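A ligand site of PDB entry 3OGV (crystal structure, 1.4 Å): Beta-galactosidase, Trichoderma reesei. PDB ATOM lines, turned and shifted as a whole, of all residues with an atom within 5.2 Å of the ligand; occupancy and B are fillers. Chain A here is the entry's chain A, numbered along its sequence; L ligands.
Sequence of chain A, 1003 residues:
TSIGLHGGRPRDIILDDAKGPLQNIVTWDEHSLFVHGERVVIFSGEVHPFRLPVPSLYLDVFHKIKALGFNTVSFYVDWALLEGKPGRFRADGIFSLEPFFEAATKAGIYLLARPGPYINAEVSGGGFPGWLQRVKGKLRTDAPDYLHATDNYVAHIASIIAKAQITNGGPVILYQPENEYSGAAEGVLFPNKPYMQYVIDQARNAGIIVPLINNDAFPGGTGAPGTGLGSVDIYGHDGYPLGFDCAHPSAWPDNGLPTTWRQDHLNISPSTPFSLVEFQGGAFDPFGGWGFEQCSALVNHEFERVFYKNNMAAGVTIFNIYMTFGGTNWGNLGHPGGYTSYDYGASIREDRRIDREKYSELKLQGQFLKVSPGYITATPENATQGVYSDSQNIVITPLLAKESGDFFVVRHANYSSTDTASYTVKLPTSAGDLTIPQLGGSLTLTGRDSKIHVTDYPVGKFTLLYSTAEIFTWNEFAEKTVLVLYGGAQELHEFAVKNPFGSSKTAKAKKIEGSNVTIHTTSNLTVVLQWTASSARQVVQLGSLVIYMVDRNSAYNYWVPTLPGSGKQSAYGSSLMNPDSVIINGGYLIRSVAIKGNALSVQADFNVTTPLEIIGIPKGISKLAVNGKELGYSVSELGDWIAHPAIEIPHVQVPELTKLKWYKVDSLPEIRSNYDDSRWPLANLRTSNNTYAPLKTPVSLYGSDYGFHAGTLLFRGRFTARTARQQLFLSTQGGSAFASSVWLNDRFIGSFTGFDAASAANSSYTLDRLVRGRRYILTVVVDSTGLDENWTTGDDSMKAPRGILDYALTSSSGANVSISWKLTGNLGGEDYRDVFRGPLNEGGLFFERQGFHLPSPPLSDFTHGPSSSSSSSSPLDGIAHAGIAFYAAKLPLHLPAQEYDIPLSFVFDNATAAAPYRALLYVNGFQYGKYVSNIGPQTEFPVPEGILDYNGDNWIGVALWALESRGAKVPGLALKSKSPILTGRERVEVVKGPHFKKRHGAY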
ATOM      1  N   TYR A  76      -2.154  -8.423   7.893  1.00  0.00           N
ATOM      2  CA  TYR A  76      -3.589  -8.032   7.976  1.00  0.00           C
ATOM      3  C   TYR A  76      -4.251  -8.612   9.152  1.00  0.00           C
ATOM      4  O   TYR A  76      -3.910  -9.715   9.666  1.00  0.00           O
ATOM      5  CB  TYR A  76      -4.326  -8.424   6.706  1.00  0.00           C
ATOM      6  CG  TYR A  76      -4.059  -7.639   5.448  1.00  0.00           C
ATOM      7  CD1 TYR A  76      -4.087  -6.194   5.448  1.00  0.00           C
ATOM      8  CD2 TYR A  76      -3.937  -8.235   4.204  1.00  0.00           C
ATOM      9  CE1 TYR A  76      -3.926  -5.509   4.242  1.00  0.00           C
ATOM     10  CE2 TYR A  76      -3.802  -7.592   3.022  1.00  0.00           C
ATOM     11  CZ  TYR A  76      -3.790  -6.164   3.072  1.00  0.00           C
ATOM     12  OH  TYR A  76      -3.598  -5.533   1.887  1.00  0.00           O
ATOM     13  N   ARG A 114      -1.729  -3.956   9.804  1.00  0.00           N
ATOM     14  CA  ARG A 114      -2.604  -3.464   8.716  1.00  0.00           C
ATOM     15  C   ARG A 114      -4.032  -4.008   9.039  1.00  0.00           C
ATOM     16  O   ARG A 114      -4.454  -5.014   8.403  1.00  0.00           O
ATOM     17  CB  ARG A 114      -2.115  -3.870   7.311  1.00  0.00           C
ATOM     18  CG  ARG A 114      -0.571  -3.642   7.193  1.00  0.00           C
ATOM     19  CD  ARG A 114      -0.108  -3.574   5.778  1.00  0.00           C
ATOM     20  NE  ARG A 114      -0.400  -4.736   4.955  1.00  0.00           N
ATOM     21  CZ  ARG A 114      -0.602  -4.724   3.661  1.00  0.00           C
ATOM     22  NH1 ARG A 114      -0.827  -3.615   2.940  1.00  0.00           N
ATOM     23  NH2 ARG A 114      -0.695  -5.891   2.967  1.00  0.00           N
ATOM     24  N   ILE A 119      -9.439  -4.806   4.004  1.00  0.00           N
ATOM     25  CA  ILE A 119      -8.059  -5.303   3.740  1.00  0.00           C
ATOM     26  C   ILE A 119      -7.926  -5.872   2.334  1.00  0.00           C
ATOM     27  O   ILE A 119      -6.785  -6.024   1.850  1.00  0.00           O
ATOM     28  CB  ILE A 119      -7.571  -6.376   4.745  1.00  0.00           C
ATOM     29  CG1 ILE A 119      -8.529  -7.607   4.765  1.00  0.00           C
ATOM     30  CG2 ILE A 119      -7.464  -5.708   6.092  1.00  0.00           C
ATOM     31  CD1 ILE A 119      -7.969  -8.855   5.536  1.00  0.00           C
ATOM     32  N   ASN A 120      -9.035  -6.164   1.580  1.00  0.00           N
ATOM     33  CA  ASN A 120      -8.971  -6.795   0.262  1.00  0.00           C
ATOM     34  C   ASN A 120      -8.444  -8.258   0.436  1.00  0.00           C
ATOM     35  O   ASN A 120      -9.176  -9.122   0.952  1.00  0.00           O
ATOM     36  CB  ASN A 120      -8.206  -5.955  -0.797  1.00  0.00           C
ATOM     37  CG  ASN A 120      -8.655  -6.242  -2.159  1.00  0.00           C
ATOM     38  OD1 ASN A 120      -9.872  -6.058  -2.496  1.00  0.00           O
ATOM     39  ND2 ASN A 120      -7.790  -6.695  -3.090  1.00  0.00           N
ATOM     40  N   ALA A 121      -7.112  -8.511   0.129  1.00  0.00           N
ATOM     41  CA  ALA A 121      -6.384  -9.710   0.658  1.00  0.00           C
ATOM     42  C   ALA A 121      -6.893 -11.017   0.046  1.00  0.00           C
ATOM     43  O   ALA A 121      -6.489 -12.096   0.564  1.00  0.00           O
ATOM     44  CB  ALA A 121      -6.423  -9.760   2.188  1.00  0.00           C
ATOM     45  N   GLU A 122      -7.765 -10.994  -0.952  1.00  0.00           N
ATOM     46  CA  GLU A 122      -8.387 -12.202  -1.494  1.00  0.00           C
ATOM     47  C   GLU A 122      -9.168 -12.926  -0.382  1.00  0.00           C
ATOM     48  O   GLU A 122      -9.286 -14.190  -0.456  1.00  0.00           O
ATOM     49  CB  GLU A 122      -7.391 -13.088  -2.285  1.00  0.00           C
ATOM     50  CG  GLU A 122      -6.958 -12.447  -3.583  1.00  0.00           C
ATOM     51  CD  GLU A 122      -5.965 -11.311  -3.428  1.00  0.00           C
ATOM     52  OE1 GLU A 122      -4.884 -11.522  -2.871  1.00  0.00           O
ATOM     53  OE2 GLU A 122      -6.242 -10.183  -3.916  1.00  0.00           O
ATOM     54  N   ASN A 179      -6.860   0.435   3.060  1.00  0.00           N
ATOM     55  CA  ASN A 179      -6.064  -0.417   2.138  1.00  0.00           C
ATOM     56  C   ASN A 179      -6.201   0.017   0.753  1.00  0.00           C
ATOM     57  O   ASN A 179      -7.314  -0.086   0.178  1.00  0.00           O
ATOM     58  CB  ASN A 179      -6.456  -1.918   2.324  1.00  0.00           C
ATOM     59  CG  ASN A 179      -5.488  -2.775   1.564  1.00  0.00           C
ATOM     60  OD1 ASN A 179      -4.347  -2.967   2.046  1.00  0.00           O
ATOM     61  ND2 ASN A 179      -5.840  -3.251   0.399  1.00  0.00           N
ATOM     62  N   GLU A 180      -5.141   0.397   0.089  1.00  0.00           N
ATOM     63  CA  GLU A 180      -5.075   0.668  -1.316  1.00  0.00           C
ATOM     64  C   GLU A 180      -6.275   1.577  -1.740  1.00  0.00           C
ATOM     65  O   GLU A 180      -7.047   1.312  -2.655  1.00  0.00           O
ATOM     66  CB  GLU A 180      -5.014  -0.641  -2.130  1.00  0.00           C
ATOM     67  CG  GLU A 180      -4.840  -0.475  -3.585  1.00  0.00           C
ATOM     68  CD  GLU A 180      -6.073  -0.768  -4.402  1.00  0.00           C
ATOM     69  OE1 GLU A 180      -6.976  -1.524  -3.964  1.00  0.00           O
ATOM     70  OE2 GLU A 180      -6.188  -0.175  -5.527  1.00  0.00           O
ATOM     71  N   ASN A 215      -0.639   2.541   1.205  1.00  0.00           N
ATOM     72  CA  ASN A 215      -0.288   1.545   0.215  1.00  0.00           C
ATOM     73  C   ASN A 215      -1.036   1.789  -1.074  1.00  0.00           C
ATOM     74  O   ASN A 215      -1.797   0.962  -1.553  1.00  0.00           O
ATOM     75  CB  ASN A 215      -0.385   0.069   0.736  1.00  0.00           C
ATOM     76  CG  ASN A 215      -1.867  -0.341   0.952  1.00  0.00           C
ATOM     77  OD1 ASN A 215      -2.653   0.446   1.497  1.00  0.00           O
ATOM     78  ND2 ASN A 215      -2.148  -1.592   0.635  1.00  0.00           N
ATOM     79  N   ALA A 217      -2.107   2.041  -4.916  1.00  0.00           N
ATOM     80  CA  ALA A 217      -1.865   1.073  -5.941  1.00  0.00           C
ATOM     81  C   ALA A 217      -0.755   1.432  -6.867  1.00  0.00           C
ATOM     82  O   ALA A 217      -0.099   0.533  -7.407  1.00  0.00           O
ATOM     83  CB  ALA A 217      -3.155   0.792  -6.757  1.00  0.00           C
ATOM     84  N   ASP A 238       2.415   0.487  -4.099  1.00  0.00           N
ATOM     85  CA  ASP A 238       2.534  -0.963  -4.354  1.00  0.00           C
ATOM     86  C   ASP A 238       3.197  -1.181  -5.701  1.00  0.00           C
ATOM     87  O   ASP A 238       3.385  -0.272  -6.512  1.00  0.00           O
ATOM     88  CB  ASP A 238       1.089  -1.572  -4.388  1.00  0.00           C
ATOM     89  CG  ASP A 238       0.364  -1.304  -3.111  1.00  0.00           C
ATOM     90  OD1 ASP A 238       0.936  -1.137  -2.039  1.00  0.00           O
ATOM     91  OD2 ASP A 238      -0.927  -1.024  -3.320  1.00  0.00           O
ATOM     92  N   GLY A 239       3.506  -2.469  -5.997  1.00  0.00           N
ATOM     93  CA  GLY A 239       3.987  -2.839  -7.274  1.00  0.00           C
ATOM     94  C   GLY A 239       3.716  -4.314  -7.557  1.00  0.00           C
ATOM     95  O   GLY A 239       4.193  -5.135  -6.819  1.00  0.00           O
ATOM     96  N   TYR A 240       2.991  -4.574  -8.646  1.00  0.00           N
ATOM     97  CA  TYR A 240       2.784  -5.937  -9.100  1.00  0.00           C
ATOM     98  C   TYR A 240       3.011  -5.948 -10.606  1.00  0.00           C
ATOM     99  O   TYR A 240       2.082  -6.059 -11.432  1.00  0.00           O
ATOM    100  CB  TYR A 240       1.372  -6.463  -8.729  1.00  0.00           C
ATOM    101  CG  TYR A 240       1.170  -6.616  -7.263  1.00  0.00           C
ATOM    102  CD1 TYR A 240       0.707  -5.580  -6.481  1.00  0.00           C
ATOM    103  CD2 TYR A 240       1.507  -7.811  -6.634  1.00  0.00           C
ATOM    104  CE1 TYR A 240       0.494  -5.745  -5.094  1.00  0.00           C
ATOM    105  CE2 TYR A 240       1.238  -8.022  -5.271  1.00  0.00           C
ATOM    106  CZ  TYR A 240       0.766  -6.953  -4.501  1.00  0.00           C
ATOM    107  OH  TYR A 240       0.553  -7.192  -3.159  1.00  0.00           O
ATOM    108  N   PHE A 244      -1.232 -10.764 -12.339  1.00  0.00           N
ATOM    109  CA  PHE A 244      -1.652 -11.894 -11.522  1.00  0.00           C
ATOM    110  C   PHE A 244      -2.023 -13.126 -12.277  1.00  0.00           C
ATOM    111  O   PHE A 244      -2.422 -14.131 -11.619  1.00  0.00           O
ATOM    112  CB  PHE A 244      -2.812 -11.496 -10.581  1.00  0.00           C
ATOM    113  CG  PHE A 244      -2.519 -10.333  -9.738  1.00  0.00           C
ATOM    114  CD1 PHE A 244      -2.958  -9.040 -10.097  1.00  0.00           C
ATOM    115  CD2 PHE A 244      -1.640 -10.481  -8.592  1.00  0.00           C
ATOM    116  CE1 PHE A 244      -2.638  -7.967  -9.229  1.00  0.00           C
ATOM    117  CE2 PHE A 244      -1.352  -9.383  -7.764  1.00  0.00           C
ATOM    118  CZ  PHE A 244      -1.829  -8.176  -8.106  1.00  0.00           C
ATOM    119  N   GLU A 278       3.608  -2.923  -0.616  1.00  0.00           N
ATOM    120  CA  GLU A 278       3.399  -4.288  -1.120  1.00  0.00           C
ATOM    121  C   GLU A 278       4.151  -4.348  -2.391  1.00  0.00           C
ATOM    122  O   GLU A 278       3.939  -3.565  -3.352  1.00  0.00           O
ATOM    123  CB  GLU A 278       1.927  -4.602  -1.411  1.00  0.00           C
ATOM    124  CG  GLU A 278       1.042  -4.509  -0.215  1.00  0.00           C
ATOM    125  CD  GLU A 278      -0.409  -4.698  -0.677  1.00  0.00           C
ATOM    126  OE1 GLU A 278      -0.678  -5.378  -1.642  1.00  0.00           O
ATOM    127  OE2 GLU A 278      -1.259  -4.274   0.115  1.00  0.00           O
ATOM    128  N   PHE A 284      -2.054 -14.284  -6.843  1.00  0.00           N
ATOM    129  CA  PHE A 284      -3.263 -15.092  -6.475  1.00  0.00           C
ATOM    130  C   PHE A 284      -3.634 -15.943  -7.716  1.00  0.00           C
ATOM    131  O   PHE A 284      -3.107 -15.774  -8.809  1.00  0.00           O
ATOM    132  CB  PHE A 284      -4.427 -14.169  -5.989  1.00  0.00           C
ATOM    133  CG  PHE A 284      -4.836 -13.112  -6.987  1.00  0.00           C
ATOM    134  CD1 PHE A 284      -5.515 -13.426  -8.175  1.00  0.00           C
ATOM    135  CD2 PHE A 284      -4.594 -11.772  -6.694  1.00  0.00           C
ATOM    136  CE1 PHE A 284      -5.905 -12.394  -9.112  1.00  0.00           C
ATOM    137  CE2 PHE A 284      -5.025 -10.739  -7.579  1.00  0.00           C
ATOM    138  CZ  PHE A 284      -5.724 -11.060  -8.765  1.00  0.00           C
ATOM    139  N   TYR A 322       4.802  -9.137  -0.677  1.00  0.00           N
ATOM    140  CA  TYR A 322       3.430  -9.680  -0.498  1.00  0.00           C
ATOM    141  C   TYR A 322       3.247 -10.768  -1.583  1.00  0.00           C
ATOM    142  O   TYR A 322       3.324 -10.484  -2.779  1.00  0.00           O
ATOM    143  CB  TYR A 322       2.433  -8.535  -0.798  1.00  0.00           C
ATOM    144  CG  TYR A 322       0.970  -8.984  -0.529  1.00  0.00           C
ATOM    145  CD1 TYR A 322       0.339  -9.878  -1.382  1.00  0.00           C
ATOM    146  CD2 TYR A 322       0.292  -8.519   0.592  1.00  0.00           C
ATOM    147  CE1 TYR A 322      -0.986 -10.326  -1.071  1.00  0.00           C
ATOM    148  CE2 TYR A 322      -1.042  -8.932   0.901  1.00  0.00           C
ATOM    149  CZ  TYR A 322      -1.599  -9.894   0.049  1.00  0.00           C
ATOM    150  OH  TYR A 322      -2.901 -10.331   0.408  1.00  0.00           O
ATOM    151  N   TYR A 342      -3.823 -20.641  -0.363  1.00  0.00           N
ATOM    152  CA  TYR A 342      -3.280 -19.257  -0.600  1.00  0.00           C
ATOM    153  C   TYR A 342      -1.716 -19.391  -0.616  1.00  0.00           C
ATOM    154  O   TYR A 342      -1.011 -18.535  -0.097  1.00  0.00           O
ATOM    155  CB  TYR A 342      -3.754 -18.247   0.485  1.00  0.00           C
ATOM    156  CG  TYR A 342      -3.637 -16.810   0.016  1.00  0.00           C
ATOM    157  CD1 TYR A 342      -4.250 -16.373  -1.112  1.00  0.00           C
ATOM    158  CD2 TYR A 342      -2.890 -15.893   0.811  1.00  0.00           C
ATOM    159  CE1 TYR A 342      -4.234 -14.986  -1.512  1.00  0.00           C
ATOM    160  CE2 TYR A 342      -2.886 -14.518   0.452  1.00  0.00           C
ATOM    161  CZ  TYR A 342      -3.511 -14.124  -0.683  1.00  0.00           C
ATOM    162  OH  TYR A 342      -3.531 -12.761  -0.989  1.00  0.00           O
ATOM    163  N   TYR A 344       0.199 -18.815  -2.944  1.00  0.00           N
ATOM    164  CA  TYR A 344       0.590 -17.568  -3.587  1.00  0.00           C
ATOM    165  C   TYR A 344       1.878 -17.695  -4.451  1.00  0.00           C
ATOM    166  O   TYR A 344       2.259 -16.768  -5.093  1.00  0.00           O
ATOM    167  CB  TYR A 344       0.794 -16.398  -2.558  1.00  0.00           C
ATOM    168  CG  TYR A 344       0.455 -15.027  -3.098  1.00  0.00           C
ATOM    169  CD1 TYR A 344      -0.896 -14.590  -3.133  1.00  0.00           C
ATOM    170  CD2 TYR A 344       1.461 -14.145  -3.510  1.00  0.00           C
ATOM    171  CE1 TYR A 344      -1.205 -13.290  -3.580  1.00  0.00           C
ATOM    172  CE2 TYR A 344       1.159 -12.852  -3.957  1.00  0.00           C
ATOM    173  CZ  TYR A 344      -0.150 -12.458  -4.031  1.00  0.00           C
ATOM    174  OH  TYR A 344      -0.416 -11.214  -4.497  1.00  0.00           O
ATOM    175  N   GLU A 789     -14.947  -9.130  -2.979  1.00  0.00           N
ATOM    176  CA  GLU A 789     -14.250  -7.944  -2.490  1.00  0.00           C
ATOM    177  C   GLU A 789     -14.917  -6.678  -2.896  1.00  0.00           C
ATOM    178  O   GLU A 789     -15.924  -6.652  -3.636  1.00  0.00           O
ATOM    179  CB  GLU A 789     -12.773  -7.967  -3.081  1.00  0.00           C
ATOM    180  CG  GLU A 789     -11.915  -9.100  -2.473  1.00  0.00           C
ATOM    181  CD  GLU A 789     -10.571  -9.165  -3.194  1.00  0.00           C
ATOM    182  OE1 GLU A 789     -10.506  -8.998  -4.443  1.00  0.00           O
ATOM    183  OE2 GLU A 789      -9.624  -9.432  -2.416  1.00  0.00           O
HETATM  184  C1  LIG L   1      -3.288  -5.413  -3.315  1.00  0.00           C
HETATM  185  O1  LIG L   1      -3.489  -6.579  -4.163  1.00  0.00           O
HETATM  186  S1  LIG L   1      -3.894  -3.980  -4.286  1.00  0.00           S
HETATM  187  C2  LIG L   1      -4.027  -5.485  -2.016  1.00  0.00           C
HETATM  188  O2  LIG L   1      -3.737  -4.401  -1.177  1.00  0.00           O
HETATM  189  C3  LIG L   1      -3.835  -6.807  -1.280  1.00  0.00           C
HETATM  190  O3  LIG L   1      -4.742  -6.901  -0.222  1.00  0.00           O
HETATM  191  C4  LIG L   1      -3.943  -7.977  -2.244  1.00  0.00           C
HETATM  192  O4  LIG L   1      -5.351  -8.046  -2.625  1.00  0.00           O
HETATM  193  C5  LIG L   1      -3.096  -7.846  -3.462  1.00  0.00           C
HETATM  194  O5  LIG L   1      -2.876 -10.132  -4.011  1.00  0.00           O
HETATM  195  C6  LIG L   1      -3.207  -8.813  -4.589  1.00  0.00           C
HETATM  196  C7  LIG L   1      -2.783  -4.021  -5.719  1.00  0.00           C
HETATM  197  C8  LIG L   1      -3.229  -3.123  -6.845  1.00  0.00           C
HETATM  198  C9  LIG L   1      -2.334  -3.221  -8.011  1.00  0.00           C
HETATM  199  C10 LIG L   1      -2.574  -4.164  -9.002  1.00  0.00           C
HETATM  200  C11 LIG L   1      -1.659  -4.269 -10.069  1.00  0.00           C
HETATM  201  C12 LIG L   1      -0.516  -3.428 -10.094  1.00  0.00           C
HETATM  202  C13 LIG L   1      -0.309  -2.534  -9.068  1.00  0.00           C
HETATM  203  C14 LIG L   1      -1.146  -2.463  -8.034  1.00  0.00           C
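O4 of the ligand is in hydrogen-bond range of OE2 of Glu 122 (2.7 Å). The side-chain hydroxyl (OH) of Tyr 344 is in hydrogen-bond range of an oxygen (O5) of the ligand (2.7 Å). OH of Tyr 76 sits at hydrogen-bond distance from O3 of the ligand (2.8 Å). OE2 of Glu 278 is in hydrogen-bond range of O2 of the ligand, at 2.8 Å. O4 of the ligand sits at hydrogen-bond distance from ND2 of Asn 120, 2.8 Å away. O2 of the ligand is in hydrogen-bond range of ND2 of Asn 179, at 2.9 Å. An oxygen (O3) of the ligand sits at hydrogen-bond distance from the backbone NH of Ala 121 (2.9 Å). The backbone carbonyl oxygen (O) of Ile 119 lies within hydrogen-bond range of an oxygen (O3) of the ligand, at 3.0 Å.
OH of Tyr 76 lies within hydrogen-bond range of OE2 of Glu 278, 3.2 Å away. The side-chain hydroxyl (OH) of Tyr 76 is in hydrogen-bond range of the backbone carbonyl oxygen (O) of Ile 119 (3.2 Å). OE1 of Glu 278 sits at hydrogen-bond distance from OH of Tyr 240, 2.7 Å away. The side-chain carboxylate of Glu 278 is in salt-bridge range of the guanidinium group of Arg 114. ND2 of Asn 120 lies close to OE2 of Glu 789 (3.4 Å). ND2 of Asn 179 is in hydrogen-bond range of O of Ile 119, at 3.3 Å. The side-chain amide oxygen of Asn 179 sits at hydrogen-bond distance from the side-chain amide nitrogen of Asn 215, at 3.0 Å. OD1 of Asn 215 is in hydrogen-bond range of N of Glu 180 (2.9 Å).
Merely in contact with the ligand: Ala 217 (3.2 Å), Tyr 322 (3.5 Å), Phe 284 (3.6 Å), Glu 180 (3.7 Å), Asn 215 (3.7 Å), Tyr 240 (3.7 Å) and Phe 244 (3.7 Å). Hydrophobic or aromatic side chains that line the ligand: Tyr 76, Ala 217, Tyr 240, Phe 244, Phe 284, Tyr 322 and Tyr 344. Within 4 Å of the ligand: Tyr 76, Ile 119, Asn 120, Ala 121, Glu 122, Asn 179, Glu 180, Asn 215, Ala 217, Tyr 240, Phe 244, Glu 278, Phe 284, Tyr 322 and Tyr 344. The nearest printed residue that does not touch the ligand is Tyr 342 (4.1 Å).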
